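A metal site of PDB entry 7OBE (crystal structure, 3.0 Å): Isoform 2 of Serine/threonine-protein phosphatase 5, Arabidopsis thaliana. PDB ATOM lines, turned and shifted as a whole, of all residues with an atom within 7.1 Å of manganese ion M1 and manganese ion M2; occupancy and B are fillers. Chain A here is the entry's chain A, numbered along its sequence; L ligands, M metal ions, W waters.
The side-chain carboxylate (OD1) of Asp 248 lies within hydrogen-bond range of the backbone NH (N) of His 433 (3.2 Å). O of His 358 sits at hydrogen-bond distance from N of Ser 432, at 3.0 Å. O of Asn 275 is in hydrogen-bond range of ND1 of His 358 (2.6 Å). The backbone carbonyl oxygen of His 433 sits at hydrogen-bond distance from the guanidinium group of Arg 406 (2.7 Å). O of Trp 392 sits at hydrogen-bond distance from NE2 of His 433, at 3.1 Å. O of Val 279 is in hydrogen-bond range of ND1 of His 250, 3.0 Å away. OD1 of Asp 277 is in hydrogen-bond range of N of His 310 (2.9 Å). The backbone NH (N) of Val 249 lies within hydrogen-bond range of the backbone carbonyl oxygen (O) of Asp 277 (3.2 Å).
Within 4 Å of manganese ion M1: Asp 248, His 250, Asp 277 and His 433.
Of the 23 residues printed, 5 come within 4 Å of manganese ion M2. Along chain A the residues within 4 Å of manganese ion M2 span positions 248 to 433. The nearest printed residue that does not touch manganese ion M2 is His 310 (4.8 Å).
Manganese ion M1 is bound by OD2 of Asp 248, NE2 of His 250, water W1, OD2 of Asp 277 and CL1 of the ligand.
Manganese ion M2 is bound by NE2 of His 358 (2.1 Å), OD1 of Asn 309 (2.1 Å), ND1 of His 433 (2.2 Å), OD2 of Asp 277 (2.3 Å) and CL1 of the ligand (2.6 Å).
Water W1 lies within hydrogen-bond range of the side-chain hydroxyl of Tyr 457 (2.9 Å) and the side-chain carboxylate of Glu 81 (3.5 Å).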
ATOM      1  N   GLU A  81      13.538 -23.323   3.608  1.00  0.00           N
ATOM      2  CA  GLU A  81      12.966 -24.525   4.220  1.00  0.00           C
ATOM      3  C   GLU A  81      12.024 -25.263   3.271  1.00  0.00           C
ATOM      4  O   GLU A  81      11.159 -26.025   3.727  1.00  0.00           O
ATOM      5  CB  GLU A  81      12.254 -24.198   5.532  1.00  0.00           C
ATOM      6  CG  GLU A  81      13.189 -23.925   6.689  1.00  0.00           C
ATOM      7  CD  GLU A  81      12.555 -23.020   7.726  1.00  0.00           C
ATOM      8  OE1 GLU A  81      11.328 -23.107   7.938  1.00  0.00           O
ATOM      9  OE2 GLU A  81      13.293 -22.192   8.320  1.00  0.00           O
ATOM     10  N   ASP A 248       4.624 -17.149  13.794  1.00  0.00           N
ATOM     11  CA  ASP A 248       5.793 -17.846  14.310  1.00  0.00           C
ATOM     12  C   ASP A 248       6.683 -16.898  15.100  1.00  0.00           C
ATOM     13  O   ASP A 248       6.911 -15.750  14.692  1.00  0.00           O
ATOM     14  CB  ASP A 248       6.590 -18.458  13.160  1.00  0.00           C
ATOM     15  CG  ASP A 248       5.836 -19.568  12.462  1.00  0.00           C
ATOM     16  OD1 ASP A 248       4.593 -19.504  12.448  1.00  0.00           O
ATOM     17  OD2 ASP A 248       6.481 -20.473  11.900  1.00  0.00           O
ATOM     18  N   VAL A 249       7.182 -17.368  16.242  1.00  0.00           N
ATOM     19  CA  VAL A 249       8.205 -16.642  16.976  1.00  0.00           C
ATOM     20  C   VAL A 249       9.483 -17.432  17.155  1.00  0.00           C
ATOM     21  O   VAL A 249      10.537 -16.823  17.416  1.00  0.00           O
ATOM     22  CB  VAL A 249       7.679 -16.151  18.345  1.00  0.00           C
ATOM     23  CG1 VAL A 249       6.641 -15.059  18.149  1.00  0.00           C
ATOM     24  CG2 VAL A 249       7.103 -17.312  19.129  1.00  0.00           C
ATOM     25  N   HIS A 250       9.439 -18.761  17.013  1.00  0.00           N
ATOM     26  CA  HIS A 250      10.601 -19.645  16.983  1.00  0.00           C
ATOM     27  C   HIS A 250      11.690 -19.231  17.975  1.00  0.00           C
ATOM     28  O   HIS A 250      12.833 -18.987  17.630  1.00  0.00           O
ATOM     29  CB  HIS A 250      11.174 -19.743  15.570  1.00  0.00           C
ATOM     30  CG  HIS A 250      10.359 -20.567  14.628  1.00  0.00           C
ATOM     31  ND1 HIS A 250      10.251 -21.937  14.730  1.00  0.00           N
ATOM     32  CD2 HIS A 250       9.615 -20.219  13.540  1.00  0.00           C
ATOM     33  CE1 HIS A 250       9.472 -22.392  13.776  1.00  0.00           C
ATOM     34  NE2 HIS A 250       9.073 -21.377  13.036  1.00  0.00           N
ATOM     35  N   ASN A 275      -0.094 -18.346  16.970  1.00  0.00           N
ATOM     36  CA  ASN A 275      -0.464 -19.367  15.981  1.00  0.00           C
ATOM     37  C   ASN A 275       0.661 -20.382  15.787  1.00  0.00           C
ATOM     38  O   ASN A 275       1.186 -20.581  14.690  1.00  0.00           O
ATOM     39  CB  ASN A 275      -0.856 -18.701  14.671  1.00  0.00           C
ATOM     40  CG  ASN A 275      -1.748 -19.565  13.801  1.00  0.00           C
ATOM     41  OD1 ASN A 275      -2.447 -20.456  14.293  1.00  0.00           O
ATOM     42  ND2 ASN A 275      -1.741 -19.303  12.505  1.00  0.00           N
ATOM     43  N   GLY A 276       1.041 -21.023  16.891  1.00  0.00           N
ATOM     44  CA  GLY A 276       1.988 -22.123  16.853  1.00  0.00           C
ATOM     45  C   GLY A 276       3.412 -21.683  16.573  1.00  0.00           C
ATOM     46  O   GLY A 276       3.719 -20.515  16.367  1.00  0.00           O
ATOM     47  N   ASP A 277       4.297 -22.679  16.567  1.00  0.00           N
ATOM     48  CA  ASP A 277       5.719 -22.508  16.316  1.00  0.00           C
ATOM     49  C   ASP A 277       6.322 -21.476  17.261  1.00  0.00           C
ATOM     50  O   ASP A 277       6.893 -20.461  16.855  1.00  0.00           O
ATOM     51  CB  ASP A 277       5.972 -22.133  14.852  1.00  0.00           C
ATOM     52  CG  ASP A 277       6.161 -23.352  13.965  1.00  0.00           C
ATOM     53  OD1 ASP A 277       5.848 -24.468  14.425  1.00  0.00           O
ATOM     54  OD2 ASP A 277       6.637 -23.202  12.820  1.00  0.00           O
ATOM     55  N   VAL A 279       8.662 -22.431  19.519  1.00  0.00           N
ATOM     56  CA  VAL A 279       9.985 -22.889  19.897  1.00  0.00           C
ATOM     57  C   VAL A 279      10.778 -23.331  18.667  1.00  0.00           C
ATOM     58  O   VAL A 279      10.353 -23.086  17.529  1.00  0.00           O
ATOM     59  CB  VAL A 279       9.892 -24.029  20.934  1.00  0.00           C
ATOM     60  CG1 VAL A 279       9.114 -23.563  22.156  1.00  0.00           C
ATOM     61  CG2 VAL A 279       9.216 -25.237  20.301  1.00  0.00           C
ATOM     62  N   ARG A 281      14.571 -23.582  16.387  1.00  0.00           N
ATOM     63  CA  ARG A 281      15.230 -22.663  15.456  1.00  0.00           C
ATOM     64  C   ARG A 281      15.891 -21.508  16.198  1.00  0.00           C
ATOM     65  O   ARG A 281      17.093 -21.283  16.044  1.00  0.00           O
ATOM     66  CB  ARG A 281      14.223 -22.160  14.423  1.00  0.00           C
ATOM     67  CG  ARG A 281      14.825 -21.841  13.071  1.00  0.00           C
ATOM     68  CD  ARG A 281      15.146 -23.087  12.261  1.00  0.00           C
ATOM     69  NE  ARG A 281      13.972 -23.662  11.626  1.00  0.00           N
ATOM     70  CZ  ARG A 281      14.027 -24.528  10.621  1.00  0.00           C
ATOM     71  NH1 ARG A 281      15.195 -24.896  10.111  1.00  0.00           N
ATOM     72  NH2 ARG A 281      12.904 -25.015  10.093  1.00  0.00           N
ATOM     73  N   GLY A 308       1.785 -25.575  16.288  1.00  0.00           N
ATOM     74  CA  GLY A 308       2.519 -25.542  15.046  1.00  0.00           C
ATOM     75  C   GLY A 308       3.158 -26.887  14.735  1.00  0.00           C
ATOM     76  O   GLY A 308       3.030 -27.857  15.469  1.00  0.00           O
ATOM     77  N   ASN A 309       3.864 -26.919  13.604  1.00  0.00           N
ATOM     78  CA  ASN A 309       4.571 -28.135  13.242  1.00  0.00           C
ATOM     79  C   ASN A 309       5.794 -28.359  14.117  1.00  0.00           C
ATOM     80  O   ASN A 309       6.222 -29.504  14.277  1.00  0.00           O
ATOM     81  CB  ASN A 309       4.973 -28.097  11.772  1.00  0.00           C
ATOM     82  CG  ASN A 309       5.588 -26.775  11.377  1.00  0.00           C
ATOM     83  OD1 ASN A 309       4.984 -25.722  11.585  1.00  0.00           O
ATOM     84  ND2 ASN A 309       6.776 -26.821  10.787  1.00  0.00           N
ATOM     85  N   HIS A 310       6.353 -27.300  14.711  1.00  0.00           N
ATOM     86  CA  HIS A 310       7.552 -27.394  15.528  1.00  0.00           C
ATOM     87  C   HIS A 310       7.235 -27.635  17.002  1.00  0.00           C
ATOM     88  O   HIS A 310       8.158 -27.631  17.826  1.00  0.00           O
ATOM     89  CB  HIS A 310       8.395 -26.127  15.375  1.00  0.00           C
ATOM     90  CG  HIS A 310       9.336 -26.187  14.219  1.00  0.00           C
ATOM     91  ND1 HIS A 310      10.548 -26.853  14.267  1.00  0.00           N
ATOM     92  CD2 HIS A 310       9.248 -25.666  12.971  1.00  0.00           C
ATOM     93  CE1 HIS A 310      11.161 -26.737  13.108  1.00  0.00           C
ATOM     94  NE2 HIS A 310      10.390 -26.026  12.300  1.00  0.00           N
ATOM     95  N   HIS A 358      -2.375 -22.879  11.765  1.00  0.00           N
ATOM     96  CA  HIS A 358      -0.965 -22.568  11.565  1.00  0.00           C
ATOM     97  C   HIS A 358      -0.536 -22.841  10.127  1.00  0.00           C
ATOM     98  O   HIS A 358       0.013 -21.952   9.463  1.00  0.00           O
ATOM     99  CB  HIS A 358      -0.114 -23.383  12.538  1.00  0.00           C
ATOM    100  CG  HIS A 358       1.361 -23.234  12.318  1.00  0.00           C
ATOM    101  ND1 HIS A 358       2.072 -22.146  12.792  1.00  0.00           N
ATOM    102  CD2 HIS A 358       2.247 -24.018  11.678  1.00  0.00           C
ATOM    103  CE1 HIS A 358       3.347 -22.287  12.450  1.00  0.00           C
ATOM    104  NE2 HIS A 358       3.471 -23.409  11.782  1.00  0.00           N
ATOM    105  N   GLY A 359      -0.792 -24.048   9.629  1.00  0.00           N
ATOM    106  CA  GLY A 359      -0.370 -24.426   8.294  1.00  0.00           C
ATOM    107  C   GLY A 359      -1.328 -24.000   7.213  1.00  0.00           C
ATOM    108  O   GLY A 359      -1.026 -23.102   6.428  1.00  0.00           O
ATOM    109  N   LEU A 391      -1.286 -28.528   9.768  1.00  0.00           N
ATOM    110  CA  LEU A 391      -0.073 -28.094  10.439  1.00  0.00           C
ATOM    111  C   LEU A 391       1.088 -27.822   9.493  1.00  0.00           C
ATOM    112  O   LEU A 391       2.051 -27.165   9.902  1.00  0.00           O
ATOM    113  CB  LEU A 391       0.366 -29.144  11.468  1.00  0.00           C
ATOM    114  CG  LEU A 391      -0.361 -29.129  12.810  1.00  0.00           C
ATOM    115  CD1 LEU A 391       0.077 -30.302  13.656  1.00  0.00           C
ATOM    116  CD2 LEU A 391      -0.087 -27.825  13.531  1.00  0.00           C
ATOM    117  N   TRP A 392       1.017 -28.297   8.243  1.00  0.00           N
ATOM    118  CA  TRP A 392       2.157 -28.246   7.339  1.00  0.00           C
ATOM    119  C   TRP A 392       1.869 -27.594   5.989  1.00  0.00           C
ATOM    120  O   TRP A 392       2.823 -27.352   5.246  1.00  0.00           O
ATOM    121  CB  TRP A 392       2.689 -29.669   7.086  1.00  0.00           C
ATOM    122  CG  TRP A 392       3.565 -30.185   8.173  1.00  0.00           C
ATOM    123  CD1 TRP A 392       3.178 -30.886   9.277  1.00  0.00           C
ATOM    124  CD2 TRP A 392       4.990 -30.051   8.268  1.00  0.00           C
ATOM    125  NE1 TRP A 392       4.274 -31.193  10.056  1.00  0.00           N
ATOM    126  CE2 TRP A 392       5.397 -30.692   9.458  1.00  0.00           C
ATOM    127  CE3 TRP A 392       5.962 -29.441   7.462  1.00  0.00           C
ATOM    128  CZ2 TRP A 392       6.730 -30.740   9.855  1.00  0.00           C
ATOM    129  CZ3 TRP A 392       7.283 -29.500   7.861  1.00  0.00           C
ATOM    130  CH2 TRP A 392       7.650 -30.142   9.049  1.00  0.00           C
ATOM    131  N   ARG A 406       7.611 -28.295   0.840  1.00  0.00           N
ATOM    132  CA  ARG A 406       8.330 -28.802   2.004  1.00  0.00           C
ATOM    133  C   ARG A 406       8.450 -30.320   2.031  1.00  0.00           C
ATOM    134  O   ARG A 406       9.092 -30.869   2.940  1.00  0.00           O
ATOM    135  CB  ARG A 406       7.648 -28.336   3.290  1.00  0.00           C
ATOM    136  CG  ARG A 406       7.290 -26.864   3.315  1.00  0.00           C
ATOM    137  CD  ARG A 406       7.092 -26.377   4.742  1.00  0.00           C
ATOM    138  NE  ARG A 406       6.410 -25.080   4.785  1.00  0.00           N
ATOM    139  CZ  ARG A 406       6.834 -24.043   5.483  1.00  0.00           C
ATOM    140  NH1 ARG A 406       6.156 -22.904   5.465  1.00  0.00           N
ATOM    141  NH2 ARG A 406       7.942 -24.139   6.215  1.00  0.00           N
ATOM    142  N   SER A 432       0.161 -18.985   9.417  1.00  0.00           N
ATOM    143  CA  SER A 432       1.561 -18.585   9.573  1.00  0.00           C
ATOM    144  C   SER A 432       2.484 -19.531   8.826  1.00  0.00           C
ATOM    145  O   SER A 432       2.409 -19.638   7.595  1.00  0.00           O
ATOM    146  CB  SER A 432       1.917 -18.503  11.053  1.00  0.00           C
ATOM    147  OG  SER A 432       1.037 -17.605  11.706  1.00  0.00           O
ATOM    148  N   HIS A 433       3.398 -20.188   9.557  1.00  0.00           N
ATOM    149  CA  HIS A 433       4.162 -21.336   9.049  1.00  0.00           C
ATOM    150  C   HIS A 433       5.213 -20.966   8.006  1.00  0.00           C
ATOM    151  O   HIS A 433       6.197 -21.696   7.845  1.00  0.00           O
ATOM    152  CB  HIS A 433       3.198 -22.385   8.487  1.00  0.00           C
ATOM    153  CG  HIS A 433       3.854 -23.655   8.065  1.00  0.00           C
ATOM    154  ND1 HIS A 433       4.729 -24.346   8.882  1.00  0.00           N
ATOM    155  CD2 HIS A 433       3.738 -24.390   6.933  1.00  0.00           C
ATOM    156  CE1 HIS A 433       5.138 -25.433   8.251  1.00  0.00           C
ATOM    157  NE2 HIS A 433       4.553 -25.485   7.069  1.00  0.00           N
ATOM    158  N   GLU A 434       5.023 -19.850   7.295  1.00  0.00           N
ATOM    159  CA  GLU A 434       5.891 -19.436   6.211  1.00  0.00           C
ATOM    160  C   GLU A 434       6.472 -18.056   6.501  1.00  0.00           C
ATOM    161  O   GLU A 434       5.757 -17.146   6.908  1.00  0.00           O
ATOM    162  CB  GLU A 434       5.139 -19.400   4.875  1.00  0.00           C
ATOM    163  CG  GLU A 434       5.910 -19.945   3.688  1.00  0.00           C
ATOM    164  CD  GLU A 434       5.047 -20.071   2.432  1.00  0.00           C
ATOM    165  OE1 GLU A 434       5.495 -20.729   1.466  1.00  0.00           O
ATOM    166  OE2 GLU A 434       3.932 -19.511   2.417  1.00  0.00           O
ATOM    167  N   VAL A 435       7.782 -17.916   6.269  1.00  0.00           N
ATOM    168  CA  VAL A 435       8.443 -16.628   6.469  1.00  0.00           C
ATOM    169  C   VAL A 435       8.006 -15.660   5.374  1.00  0.00           C
ATOM    170  O   VAL A 435       7.777 -16.050   4.229  1.00  0.00           O
ATOM    171  CB  VAL A 435       9.975 -16.827   6.489  1.00  0.00           C
ATOM    172  CG1 VAL A 435      10.444 -17.477   5.197  1.00  0.00           C
ATOM    173  CG2 VAL A 435      10.693 -15.506   6.720  1.00  0.00           C
ATOM    174  N   PHE A 452       3.558 -13.560  10.443  1.00  0.00           N
ATOM    175  CA  PHE A 452       4.838 -14.142  10.860  1.00  0.00           C
ATOM    176  C   PHE A 452       5.518 -13.142  11.783  1.00  0.00           C
ATOM    177  O   PHE A 452       5.854 -12.035  11.348  1.00  0.00           O
ATOM    178  CB  PHE A 452       5.691 -14.468   9.638  1.00  0.00           C
ATOM    179  CG  PHE A 452       6.946 -15.232   9.943  1.00  0.00           C
ATOM    180  CD1 PHE A 452       8.108 -14.577  10.313  1.00  0.00           C
ATOM    181  CD2 PHE A 452       6.971 -16.615   9.835  1.00  0.00           C
ATOM    182  CE1 PHE A 452       9.266 -15.274  10.579  1.00  0.00           C
ATOM    183  CE2 PHE A 452       8.128 -17.322  10.097  1.00  0.00           C
ATOM    184  CZ  PHE A 452       9.271 -16.656  10.466  1.00  0.00           C
ATOM    185  N   TYR A 457      14.503 -13.477  10.807  1.00  0.00           N
ATOM    186  CA  TYR A 457      14.446 -14.912  11.079  1.00  0.00           C
ATOM    187  C   TYR A 457      15.838 -15.527  11.060  1.00  0.00           C
ATOM    188  O   TYR A 457      16.633 -15.276  10.146  1.00  0.00           O
ATOM    189  CB  TYR A 457      13.548 -15.581  10.036  1.00  0.00           C
ATOM    190  CG  TYR A 457      13.209 -17.030  10.302  1.00  0.00           C
ATOM    191  CD1 TYR A 457      12.859 -17.464  11.578  1.00  0.00           C
ATOM    192  CD2 TYR A 457      13.215 -17.961   9.267  1.00  0.00           C
ATOM    193  CE1 TYR A 457      12.529 -18.795  11.814  1.00  0.00           C
ATOM    194  CE2 TYR A 457      12.897 -19.289   9.497  1.00  0.00           C
ATOM    195  CZ  TYR A 457      12.549 -19.701  10.771  1.00  0.00           C
ATOM    196  OH  TYR A 457      12.234 -21.016  10.996  1.00  0.00           O
HETATM  197 CL1  LIG L   1       7.816 -24.085  10.140  1.00  0.00          CL
HETATM  198 MN    MN M   1       7.678 -21.756  11.265  1.00  0.00          MN
HETATM  199 MN    MN M   2       5.355 -23.728  10.937  1.00  0.00          MN
HETATM  200  O   HOH W   1       9.465 -21.011   9.988  1.00  0.00           O
